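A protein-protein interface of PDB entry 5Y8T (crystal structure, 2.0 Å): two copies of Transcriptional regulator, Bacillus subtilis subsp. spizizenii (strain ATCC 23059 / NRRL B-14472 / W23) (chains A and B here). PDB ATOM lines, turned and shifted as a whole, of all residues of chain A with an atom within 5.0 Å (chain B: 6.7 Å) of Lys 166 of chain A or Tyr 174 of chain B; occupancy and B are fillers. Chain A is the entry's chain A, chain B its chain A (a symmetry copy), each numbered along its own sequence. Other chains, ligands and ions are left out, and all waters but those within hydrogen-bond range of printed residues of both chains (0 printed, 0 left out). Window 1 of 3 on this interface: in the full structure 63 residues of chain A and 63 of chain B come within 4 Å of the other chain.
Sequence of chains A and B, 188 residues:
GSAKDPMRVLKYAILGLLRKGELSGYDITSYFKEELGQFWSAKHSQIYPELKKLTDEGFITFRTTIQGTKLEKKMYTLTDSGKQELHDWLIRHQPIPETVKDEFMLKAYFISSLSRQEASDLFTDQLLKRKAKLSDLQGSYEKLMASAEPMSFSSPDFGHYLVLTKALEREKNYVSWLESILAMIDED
Tyr 161 of chain A touches none of the printed residues of chain B. Of the printed residues of chain B, Val 163 of chain A touches Met 105 (3.6 Å). Printed residues of chain B within 4 Å of Thr 165 of chain A: Trp 177. Of chain B, only Met 105 (3.4 Å), Tyr 174 (3.4 Å) and Trp 177 (3.4 Å) come within 4 Å of Lys 166 of chain A. Printed residues of chain B within 4 Å of Glu 169 of chain A: Asn 173 (3.0 Å).
Of the 10 printed residues of chain A, 6 touch a printed residue of chain B. Hydrophobic or aromatic side chains of chain A within 4 Å of the printed part of chain B: Val 163. Of the 18 printed residues of chain B, 4 touch a printed residue of chain A. Hydrophobic or aromatic side chains of chain B that line the printed part of chain A: Met 105, Tyr 174 and Trp 177. Among the printed residues, 9 pairs touch across the chains. Among the printed residues, no Asp or Glu carboxylate lies within 4 Å of a Lys or Arg side-chain nitrogen of the other chain.
Positions printed for both chains: 169 and 170.
NE1 of Trp 177 of chain B lies close to N of Lys 166 of chain A, at 3.4 Å. OG1 of Thr 165 of chain A is in hydrogen-bond range of NE1 of Trp 177 of chain B. OE1 of Glu 169 of chain A sits at hydrogen-bond distance from ND2 of Asn 173 of chain B, at 3.0 Å.
OD1 of Asp 102 of chain B sits at hydrogen-bond distance from N of Met 105 of chain B, 3.3 Å away. O of Leu 162 of chain A sits at hydrogen-bond distance from OG1 of Thr 165 of chain A, at 3.4 Å. The side-chain hydroxyl of Tyr 174 of chain B sits at hydrogen-bond distance from the side-chain carboxylate of Asp 102 of chain B (2.6 Å). The side-chain hydroxyl (OG1) of Thr 165 of chain A lies within hydrogen-bond range of the backbone carbonyl oxygen (O) of Tyr 161 of chain A (2.9 Å).
Leu 162 of chain A touches Met 105 of chain B. Leu 162 of chain A touches Trp 177 of chain B. CG1 of Val 163 of chain A touches O of Met 105 of chain B, at 3.6 Å. CE of Met 105 of chain B touches CB of Lys 166 of chain A (3.4 Å). Tyr 174 of chain B touches Lys 166 of chain A (CZ to CE, 3.4 Å). Arg 170 of chain A touches Asn 173 of chain B.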
ATOM      1  N   TYR A 161      34.365 -18.781  12.146  1.00  0.00           N
ATOM      2  CA  TYR A 161      34.050 -19.332  13.476  1.00  0.00           C
ATOM      3  C   TYR A 161      32.667 -18.826  13.916  1.00  0.00           C
ATOM      4  O   TYR A 161      31.877 -19.580  14.450  1.00  0.00           O
ATOM      5  CB  TYR A 161      35.158 -18.910  14.482  1.00  0.00           C
ATOM      6  CG  TYR A 161      34.867 -19.184  15.929  1.00  0.00           C
ATOM      7  CD1 TYR A 161      35.178 -20.420  16.489  1.00  0.00           C
ATOM      8  CD2 TYR A 161      34.311 -18.227  16.742  1.00  0.00           C
ATOM      9  CE1 TYR A 161      34.938 -20.694  17.844  1.00  0.00           C
ATOM     10  CE2 TYR A 161      34.032 -18.508  18.100  1.00  0.00           C
ATOM     11  CZ  TYR A 161      34.370 -19.738  18.629  1.00  0.00           C
ATOM     12  OH  TYR A 161      34.129 -20.034  19.949  1.00  0.00           O
ATOM     13  N   LEU A 162      32.346 -17.570  13.622  1.00  0.00           N
ATOM     14  CA  LEU A 162      31.019 -17.045  14.006  1.00  0.00           C
ATOM     15  C   LEU A 162      29.879 -17.784  13.249  1.00  0.00           C
ATOM     16  O   LEU A 162      28.908 -18.192  13.855  1.00  0.00           O
ATOM     17  CB  LEU A 162      30.912 -15.543  13.770  1.00  0.00           C
ATOM     18  CG  LEU A 162      31.804 -14.660  14.641  1.00  0.00           C
ATOM     19  CD1 LEU A 162      31.472 -13.182  14.401  1.00  0.00           C
ATOM     20  CD2 LEU A 162      31.700 -15.019  16.181  1.00  0.00           C
ATOM     21  N   VAL A 163      29.988 -17.961  11.946  1.00  0.00           N
ATOM     22  CA  VAL A 163      28.893 -18.606  11.228  1.00  0.00           C
ATOM     23  C   VAL A 163      28.810 -20.092  11.595  1.00  0.00           C
ATOM     24  O   VAL A 163      27.712 -20.675  11.666  1.00  0.00           O
ATOM     25  CB  VAL A 163      28.972 -18.384   9.736  1.00  0.00           C
ATOM     26  CG1 VAL A 163      28.828 -16.926   9.399  1.00  0.00           C
ATOM     27  CG2 VAL A 163      30.279 -18.938   9.128  1.00  0.00           C
ATOM     28  N   LEU A 164      29.938 -20.723  11.878  1.00  0.00           N
ATOM     29  CA  LEU A 164      29.898 -22.150  12.216  1.00  0.00           C
ATOM     30  C   LEU A 164      29.396 -22.381  13.651  1.00  0.00           C
ATOM     31  O   LEU A 164      28.566 -23.261  13.863  1.00  0.00           O
ATOM     32  CB  LEU A 164      31.262 -22.777  11.995  1.00  0.00           C
ATOM     33  CG  LEU A 164      31.434 -24.252  12.151  1.00  0.00           C
ATOM     34  CD1 LEU A 164      30.211 -25.032  11.533  1.00  0.00           C
ATOM     35  CD2 LEU A 164      32.804 -24.590  11.446  1.00  0.00           C
ATOM     36  N   THR A 165      29.860 -21.618  14.636  1.00  0.00           N
ATOM     37  CA  THR A 165      29.302 -21.766  15.996  1.00  0.00           C
ATOM     38  C   THR A 165      27.817 -21.355  16.059  1.00  0.00           C
ATOM     39  O   THR A 165      27.036 -21.949  16.822  1.00  0.00           O
ATOM     40  CB  THR A 165      30.099 -20.955  17.077  1.00  0.00           C
ATOM     41  OG1 THR A 165      30.133 -19.573  16.712  1.00  0.00           O
ATOM     42  CG2 THR A 165      31.537 -21.459  17.187  1.00  0.00           C
ATOM     43  N   LYS A 166      27.407 -20.344  15.303  1.00  0.00           N
ATOM     44  CA  LYS A 166      25.985 -20.012  15.231  1.00  0.00           C
ATOM     45  C   LYS A 166      25.181 -21.207  14.731  1.00  0.00           C
ATOM     46  O   LYS A 166      24.166 -21.542  15.307  1.00  0.00           O
ATOM     47  CB  LYS A 166      25.728 -18.825  14.312  1.00  0.00           C
ATOM     48  CG  LYS A 166      24.243 -18.401  14.246  1.00  0.00           C
ATOM     49  CD  LYS A 166      23.833 -17.730  15.567  1.00  0.00           C
ATOM     50  CE  LYS A 166      22.390 -17.345  15.578  1.00  0.00           C
ATOM     51  NZ  LYS A 166      21.564 -18.542  15.823  1.00  0.00           N
ATOM     52  N   ALA A 167      25.656 -21.863  13.677  1.00  0.00           N
ATOM     53  CA  ALA A 167      24.945 -23.027  13.121  1.00  0.00           C
ATOM     54  C   ALA A 167      24.964 -24.203  14.097  1.00  0.00           C
ATOM     55  O   ALA A 167      23.956 -24.857  14.309  1.00  0.00           O
ATOM     56  CB  ALA A 167      25.523 -23.412  11.751  1.00  0.00           C
ATOM     57  N   LEU A 168      26.080 -24.418  14.765  1.00  0.00           N
ATOM     58  CA  LEU A 168      26.166 -25.448  15.817  1.00  0.00           C
ATOM     59  C   LEU A 168      25.155 -25.203  16.934  1.00  0.00           C
ATOM     60  O   LEU A 168      24.398 -26.102  17.349  1.00  0.00           O
ATOM     61  CB  LEU A 168      27.599 -25.496  16.393  1.00  0.00           C
ATOM     62  CG  LEU A 168      28.662 -26.237  15.564  1.00  0.00           C
ATOM     63  CD1 LEU A 168      30.065 -25.815  16.021  1.00  0.00           C
ATOM     64  CD2 LEU A 168      28.464 -27.788  15.655  1.00  0.00           C
ATOM     65  N   GLU A 169      25.126 -23.988  17.428  1.00  0.00           N
ATOM     66  CA  GLU A 169      24.216 -23.665  18.523  1.00  0.00           C
ATOM     67  C   GLU A 169      22.762 -23.786  18.090  1.00  0.00           C
ATOM     68  O   GLU A 169      21.949 -24.355  18.827  1.00  0.00           O
ATOM     69  CB  GLU A 169      24.497 -22.275  19.083  1.00  0.00           C
ATOM     70  CG  GLU A 169      25.693 -22.262  19.970  1.00  0.00           C
ATOM     71  CD  GLU A 169      25.444 -23.076  21.243  1.00  0.00           C
ATOM     72  OE1 GLU A 169      24.429 -22.808  21.908  1.00  0.00           O
ATOM     73  OE2 GLU A 169      26.234 -23.996  21.529  1.00  0.00           O
ATOM     74  N   ARG A 170      22.449 -23.343  16.864  1.00  0.00           N
ATOM     75  CA  ARG A 170      21.098 -23.443  16.333  1.00  0.00           C
ATOM     76  C   ARG A 170      20.608 -24.878  16.251  1.00  0.00           C
ATOM     77  O   ARG A 170      19.505 -25.139  16.640  1.00  0.00           O
ATOM     78  CB  ARG A 170      21.019 -22.800  14.942  1.00  0.00           C
ATOM     79  CG  ARG A 170      19.631 -22.695  14.307  1.00  0.00           C
ATOM     80  CD  ARG A 170      19.816 -22.119  12.848  1.00  0.00           C
ATOM     81  NE  ARG A 170      20.522 -23.181  12.131  1.00  0.00           N
ATOM     82  CZ  ARG A 170      21.456 -23.053  11.191  1.00  0.00           C
ATOM     83  NH1 ARG A 170      21.848 -21.878  10.763  1.00  0.00           N
ATOM     84  NH2 ARG A 170      22.035 -24.155  10.691  1.00  0.00           N
ATOM     85  N   ASP B 102      20.318 -15.449   7.136  1.00  0.00           N
ATOM     86  CA  ASP B 102      20.221 -14.508   8.219  1.00  0.00           C
ATOM     87  C   ASP B 102      21.221 -13.418   7.844  1.00  0.00           C
ATOM     88  O   ASP B 102      22.437 -13.632   7.845  1.00  0.00           O
ATOM     89  CB  ASP B 102      20.534 -15.237   9.513  1.00  0.00           C
ATOM     90  CG  ASP B 102      20.563 -14.318  10.733  1.00  0.00           C
ATOM     91  OD1 ASP B 102      20.846 -13.145  10.565  1.00  0.00           O
ATOM     92  OD2 ASP B 102      20.366 -14.819  11.843  1.00  0.00           O
ATOM     93  N   GLU B 103      20.695 -12.249   7.488  1.00  0.00           N
ATOM     94  CA  GLU B 103      21.514 -11.154   7.027  1.00  0.00           C
ATOM     95  C   GLU B 103      22.508 -10.696   8.108  1.00  0.00           C
ATOM     96  O   GLU B 103      23.634 -10.318   7.786  1.00  0.00           O
ATOM     97  CB  GLU B 103      20.653  -9.961   6.557  1.00  0.00           C
ATOM     98  CG  GLU B 103      21.482  -8.909   5.855  1.00  0.00           C
ATOM     99  CD  GLU B 103      20.664  -7.877   5.073  1.00  0.00           C
ATOM    100  OE1 GLU B 103      21.194  -7.288   4.108  1.00  0.00           O
ATOM    101  OE2 GLU B 103      19.509  -7.644   5.421  1.00  0.00           O
ATOM    102  N   PHE B 104      22.108 -10.746   9.375  1.00  0.00           N
ATOM    103  CA  PHE B 104      23.061 -10.439  10.460  1.00  0.00           C
ATOM    104  C   PHE B 104      24.298 -11.363  10.408  1.00  0.00           C
ATOM    105  O   PHE B 104      25.413 -10.933  10.619  1.00  0.00           O
ATOM    106  CB  PHE B 104      22.395 -10.543  11.830  1.00  0.00           C
ATOM    107  CG  PHE B 104      23.353 -10.288  12.952  1.00  0.00           C
ATOM    108  CD1 PHE B 104      23.733  -8.986  13.248  1.00  0.00           C
ATOM    109  CD2 PHE B 104      23.937 -11.329  13.636  1.00  0.00           C
ATOM    110  CE1 PHE B 104      24.657  -8.732  14.231  1.00  0.00           C
ATOM    111  CE2 PHE B 104      24.883 -11.079  14.638  1.00  0.00           C
ATOM    112  CZ  PHE B 104      25.237  -9.773  14.934  1.00  0.00           C
ATOM    113  N   MET B 105      24.069 -12.634  10.116  1.00  0.00           N
ATOM    114  CA  MET B 105      25.155 -13.606  10.100  1.00  0.00           C
ATOM    115  C   MET B 105      26.106 -13.407   8.954  1.00  0.00           C
ATOM    116  O   MET B 105      27.270 -13.736   9.076  1.00  0.00           O
ATOM    117  CB  MET B 105      24.575 -15.020  10.179  1.00  0.00           C
ATOM    118  CG  MET B 105      24.007 -15.338  11.575  1.00  0.00           C
ATOM    119  SD  MET B 105      25.072 -15.064  12.984  1.00  0.00           S
ATOM    120  CE  MET B 105      26.528 -16.023  12.507  1.00  0.00           C
ATOM    121  N   GLN B 126      22.211  -6.059  18.069  1.00  0.00           N
ATOM    122  CA  GLN B 126      21.507  -7.307  17.771  1.00  0.00           C
ATOM    123  C   GLN B 126      21.032  -7.984  19.066  1.00  0.00           C
ATOM    124  O   GLN B 126      19.927  -8.544  19.133  1.00  0.00           O
ATOM    125  CB  GLN B 126      22.413  -8.242  16.958  1.00  0.00           C
ATOM    126  CG  GLN B 126      21.730  -9.503  16.454  1.00  0.00           C
ATOM    127  CD  GLN B 126      20.687  -9.246  15.334  1.00  0.00           C
ATOM    128  OE1 GLN B 126      19.841 -10.115  15.052  1.00  0.00           O
ATOM    129  NE2 GLN B 126      20.762  -8.081  14.689  1.00  0.00           N
ATOM    130  N   LEU B 127      21.858  -7.927  20.116  1.00  0.00           N
ATOM    131  CA  LEU B 127      21.541  -8.582  21.371  1.00  0.00           C
ATOM    132  C   LEU B 127      20.299  -7.898  21.980  1.00  0.00           C
ATOM    133  O   LEU B 127      19.373  -8.578  22.498  1.00  0.00           O
ATOM    134  CB  LEU B 127      22.739  -8.497  22.334  1.00  0.00           C
ATOM    135  CG  LEU B 127      22.472  -9.003  23.753  1.00  0.00           C
ATOM    136  CD1 LEU B 127      22.108 -10.512  23.701  1.00  0.00           C
ATOM    137  CD2 LEU B 127      23.689  -8.714  24.684  1.00  0.00           C
ATOM    138  N   ARG B 130      17.181  -9.050  20.036  1.00  0.00           N
ATOM    139  CA  ARG B 130      16.789 -10.432  20.283  1.00  0.00           C
ATOM    140  C   ARG B 130      16.186 -10.603  21.650  1.00  0.00           C
ATOM    141  O   ARG B 130      15.238 -11.337  21.808  1.00  0.00           O
ATOM    142  CB  ARG B 130      17.959 -11.408  20.122  1.00  0.00           C
ATOM    143  CG  ARG B 130      18.533 -11.395  18.735  1.00  0.00           C
ATOM    144  CD  ARG B 130      17.879 -12.378  17.848  1.00  0.00           C
ATOM    145  NE  ARG B 130      18.162 -12.115  16.461  1.00  0.00           N
ATOM    146  CZ  ARG B 130      17.411 -12.566  15.472  1.00  0.00           C
ATOM    147  NH1 ARG B 130      16.370 -13.367  15.721  1.00  0.00           N
ATOM    148  NH2 ARG B 130      17.697 -12.225  14.230  1.00  0.00           N
ATOM    149  N   GLU B 169      12.834 -20.919  22.484  1.00  0.00           N
ATOM    150  CA  GLU B 169      14.133 -21.582  22.542  1.00  0.00           C
ATOM    151  C   GLU B 169      15.088 -21.024  21.496  1.00  0.00           C
ATOM    152  O   GLU B 169      16.256 -20.765  21.809  1.00  0.00           O
ATOM    153  CB  GLU B 169      13.989 -23.092  22.388  1.00  0.00           C
ATOM    154  CG  GLU B 169      13.517 -23.738  23.645  1.00  0.00           C
ATOM    155  CD  GLU B 169      14.569 -23.626  24.752  1.00  0.00           C
ATOM    156  OE1 GLU B 169      15.721 -24.014  24.492  1.00  0.00           O
ATOM    157  OE2 GLU B 169      14.242 -23.111  25.838  1.00  0.00           O
ATOM    158  N   ARG B 170      14.579 -20.749  20.287  1.00  0.00           N
ATOM    159  CA  ARG B 170      15.392 -20.178  19.223  1.00  0.00           C
ATOM    160  C   ARG B 170      15.981 -18.829  19.599  1.00  0.00           C
ATOM    161  O   ARG B 170      17.136 -18.614  19.366  1.00  0.00           O
ATOM    162  CB  ARG B 170      14.567 -20.030  17.937  1.00  0.00           C
ATOM    163  CG  ARG B 170      15.318 -19.578  16.683  1.00  0.00           C
ATOM    164  CD  ARG B 170      14.252 -19.384  15.534  1.00  0.00           C
ATOM    165  NE  ARG B 170      13.453 -18.240  15.976  1.00  0.00           N
ATOM    166  CZ  ARG B 170      12.147 -18.042  15.813  1.00  0.00           C
ATOM    167  NH1 ARG B 170      11.393 -18.901  15.171  1.00  0.00           N
ATOM    168  NH2 ARG B 170      11.579 -16.951  16.347  1.00  0.00           N
ATOM    169  N   GLU B 171      15.174 -17.910  20.152  1.00  0.00           N
ATOM    170  CA  GLU B 171      15.666 -16.593  20.527  1.00  0.00           C
ATOM    171  C   GLU B 171      16.540 -16.634  21.776  1.00  0.00           C
ATOM    172  O   GLU B 171      17.537 -15.903  21.845  1.00  0.00           O
ATOM    173  CB  GLU B 171      14.505 -15.612  20.704  1.00  0.00           C
ATOM    174  CG  GLU B 171      13.676 -15.430  19.464  1.00  0.00           C
ATOM    175  CD  GLU B 171      14.474 -15.039  18.211  1.00  0.00           C
ATOM    176  OE1 GLU B 171      15.487 -14.335  18.347  1.00  0.00           O
ATOM    177  OE2 GLU B 171      14.061 -15.402  17.091  1.00  0.00           O
ATOM    178  N   LYS B 172      16.204 -17.487  22.766  1.00  0.00           N
ATOM    179  CA  LYS B 172      17.104 -17.684  23.936  1.00  0.00           C
ATOM    180  C   LYS B 172      18.478 -18.147  23.478  1.00  0.00           C
ATOM    181  O   LYS B 172      19.529 -17.657  23.981  1.00  0.00           O
ATOM    182  CB  LYS B 172      16.563 -18.705  24.958  1.00  0.00           C
ATOM    183  CG  LYS B 172      15.372 -18.161  25.796  1.00  0.00           C
ATOM    184  CD  LYS B 172      14.678 -19.273  26.632  1.00  0.00           C
ATOM    185  CE  LYS B 172      13.392 -18.748  27.260  1.00  0.00           C
ATOM    186  NZ  LYS B 172      12.771 -19.743  28.168  1.00  0.00           N
ATOM    187  N   ASN B 173      18.478 -19.079  22.529  1.00  0.00           N
ATOM    188  CA  ASN B 173      19.742 -19.601  22.022  1.00  0.00           C
ATOM    189  C   ASN B 173      20.536 -18.519  21.268  1.00  0.00           C
ATOM    190  O   ASN B 173      21.736 -18.424  21.404  1.00  0.00           O
ATOM    191  CB  ASN B 173      19.507 -20.823  21.136  1.00  0.00           C
ATOM    192  CG  ASN B 173      20.823 -21.397  20.593  1.00  0.00           C
ATOM    193  OD1 ASN B 173      21.154 -21.211  19.421  1.00  0.00           O
ATOM    194  ND2 ASN B 173      21.536 -22.088  21.429  1.00  0.00           N
ATOM    195  N   TYR B 174      19.845 -17.672  20.514  1.00  0.00           N
ATOM    196  CA  TYR B 174      20.487 -16.593  19.785  1.00  0.00           C
ATOM    197  C   TYR B 174      21.117 -15.600  20.772  1.00  0.00           C
ATOM    198  O   TYR B 174      22.269 -15.193  20.613  1.00  0.00           O
ATOM    199  CB  TYR B 174      19.447 -15.950  18.869  1.00  0.00           C
ATOM    200  CG  TYR B 174      19.935 -15.385  17.553  1.00  0.00           C
ATOM    201  CD1 TYR B 174      21.063 -14.562  17.492  1.00  0.00           C
ATOM    202  CD2 TYR B 174      19.257 -15.656  16.363  1.00  0.00           C
ATOM    203  CE1 TYR B 174      21.501 -14.023  16.298  1.00  0.00           C
ATOM    204  CE2 TYR B 174      19.681 -15.127  15.156  1.00  0.00           C
ATOM    205  CZ  TYR B 174      20.831 -14.303  15.128  1.00  0.00           C
ATOM    206  OH  TYR B 174      21.316 -13.752  13.960  1.00  0.00           O
ATOM    207  N   VAL B 175      20.344 -15.198  21.770  1.00  0.00           N
ATOM    208  CA  VAL B 175      20.818 -14.327  22.840  1.00  0.00           C
ATOM    209  C   VAL B 175      22.059 -14.895  23.518  1.00  0.00           C
ATOM    210  O   VAL B 175      23.045 -14.179  23.702  1.00  0.00           O
ATOM    211  CB  VAL B 175      19.699 -14.064  23.884  1.00  0.00           C
ATOM    212  CG1 VAL B 175      20.291 -13.459  25.166  1.00  0.00           C
ATOM    213  CG2 VAL B 175      18.611 -13.173  23.253  1.00  0.00           C
ATOM    214  N   SER B 176      22.029 -16.181  23.864  1.00  0.00           N
ATOM    215  CA  SER B 176      23.178 -16.855  24.475  1.00  0.00           C
ATOM    216  C   SER B 176      24.431 -16.829  23.584  1.00  0.00           C
ATOM    217  O   SER B 176      25.534 -16.493  24.036  1.00  0.00           O
ATOM    218  CB  SER B 176      22.851 -18.321  24.812  1.00  0.00           C
ATOM    219  OG  SER B 176      23.930 -18.856  25.547  1.00  0.00           O
ATOM    220  N   TRP B 177      24.244 -17.120  22.305  1.00  0.00           N
ATOM    221  CA  TRP B 177      25.360 -17.089  21.392  1.00  0.00           C
ATOM    222  C   TRP B 177      25.889 -15.653  21.284  1.00  0.00           C
ATOM    223  O   TRP B 177      27.065 -15.424  21.335  1.00  0.00           O
ATOM    224  CB  TRP B 177      24.889 -17.565  20.034  1.00  0.00           C
ATOM    225  CG  TRP B 177      25.942 -17.525  19.016  1.00  0.00           C
ATOM    226  CD1 TRP B 177      26.922 -18.457  18.835  1.00  0.00           C
ATOM    227  CD2 TRP B 177      26.170 -16.516  18.062  1.00  0.00           C
ATOM    228  NE1 TRP B 177      27.722 -18.101  17.810  1.00  0.00           N
ATOM    229  CE2 TRP B 177      27.292 -16.908  17.307  1.00  0.00           C
ATOM    230  CE3 TRP B 177      25.509 -15.337  17.717  1.00  0.00           C
ATOM    231  CZ2 TRP B 177      27.779 -16.154  16.251  1.00  0.00           C
ATOM    232  CZ3 TRP B 177      26.021 -14.571  16.690  1.00  0.00           C
ATOM    233  CH2 TRP B 177      27.159 -14.984  15.971  1.00  0.00           C
ATOM    234  N   LEU B 178      25.006 -14.671  21.161  1.00  0.00           N
ATOM    235  CA  LEU B 178      25.445 -13.258  21.089  1.00  0.00           C
ATOM    236  C   LEU B 178      26.218 -12.803  22.313  1.00  0.00           C
ATOM    237  O   LEU B 178      27.244 -12.175  22.168  1.00  0.00           O
ATOM    238  CB  LEU B 178      24.262 -12.335  20.860  1.00  0.00           C
ATOM    239  CG  LEU B 178      23.690 -12.332  19.469  1.00  0.00           C
ATOM    240  CD1 LEU B 178      22.256 -11.767  19.511  1.00  0.00           C
ATOM    241  CD2 LEU B 178      24.555 -11.518  18.532  1.00  0.00           C
ATOM    242  N   GLU B 179      25.747 -13.154  23.506  1.00  0.00           N
ATOM    243  CA  GLU B 179      26.478 -12.893  24.719  1.00  0.00           C
ATOM    244  C   GLU B 179      27.856 -13.525  24.742  1.00  0.00           C
ATOM    245  O   GLU B 179      28.811 -12.900  25.227  1.00  0.00           O
ATOM    246  CB  GLU B 179      25.684 -13.337  25.947  1.00  0.00           C
ATOM    247  CG  GLU B 179      24.496 -12.421  26.192  1.00  0.00           C
ATOM    248  CD  GLU B 179      23.479 -12.972  27.202  1.00  0.00           C
ATOM    249  OE1 GLU B 179      23.520 -14.182  27.550  1.00  0.00           O
ATOM    250  OE2 GLU B 179      22.608 -12.175  27.639  1.00  0.00           O
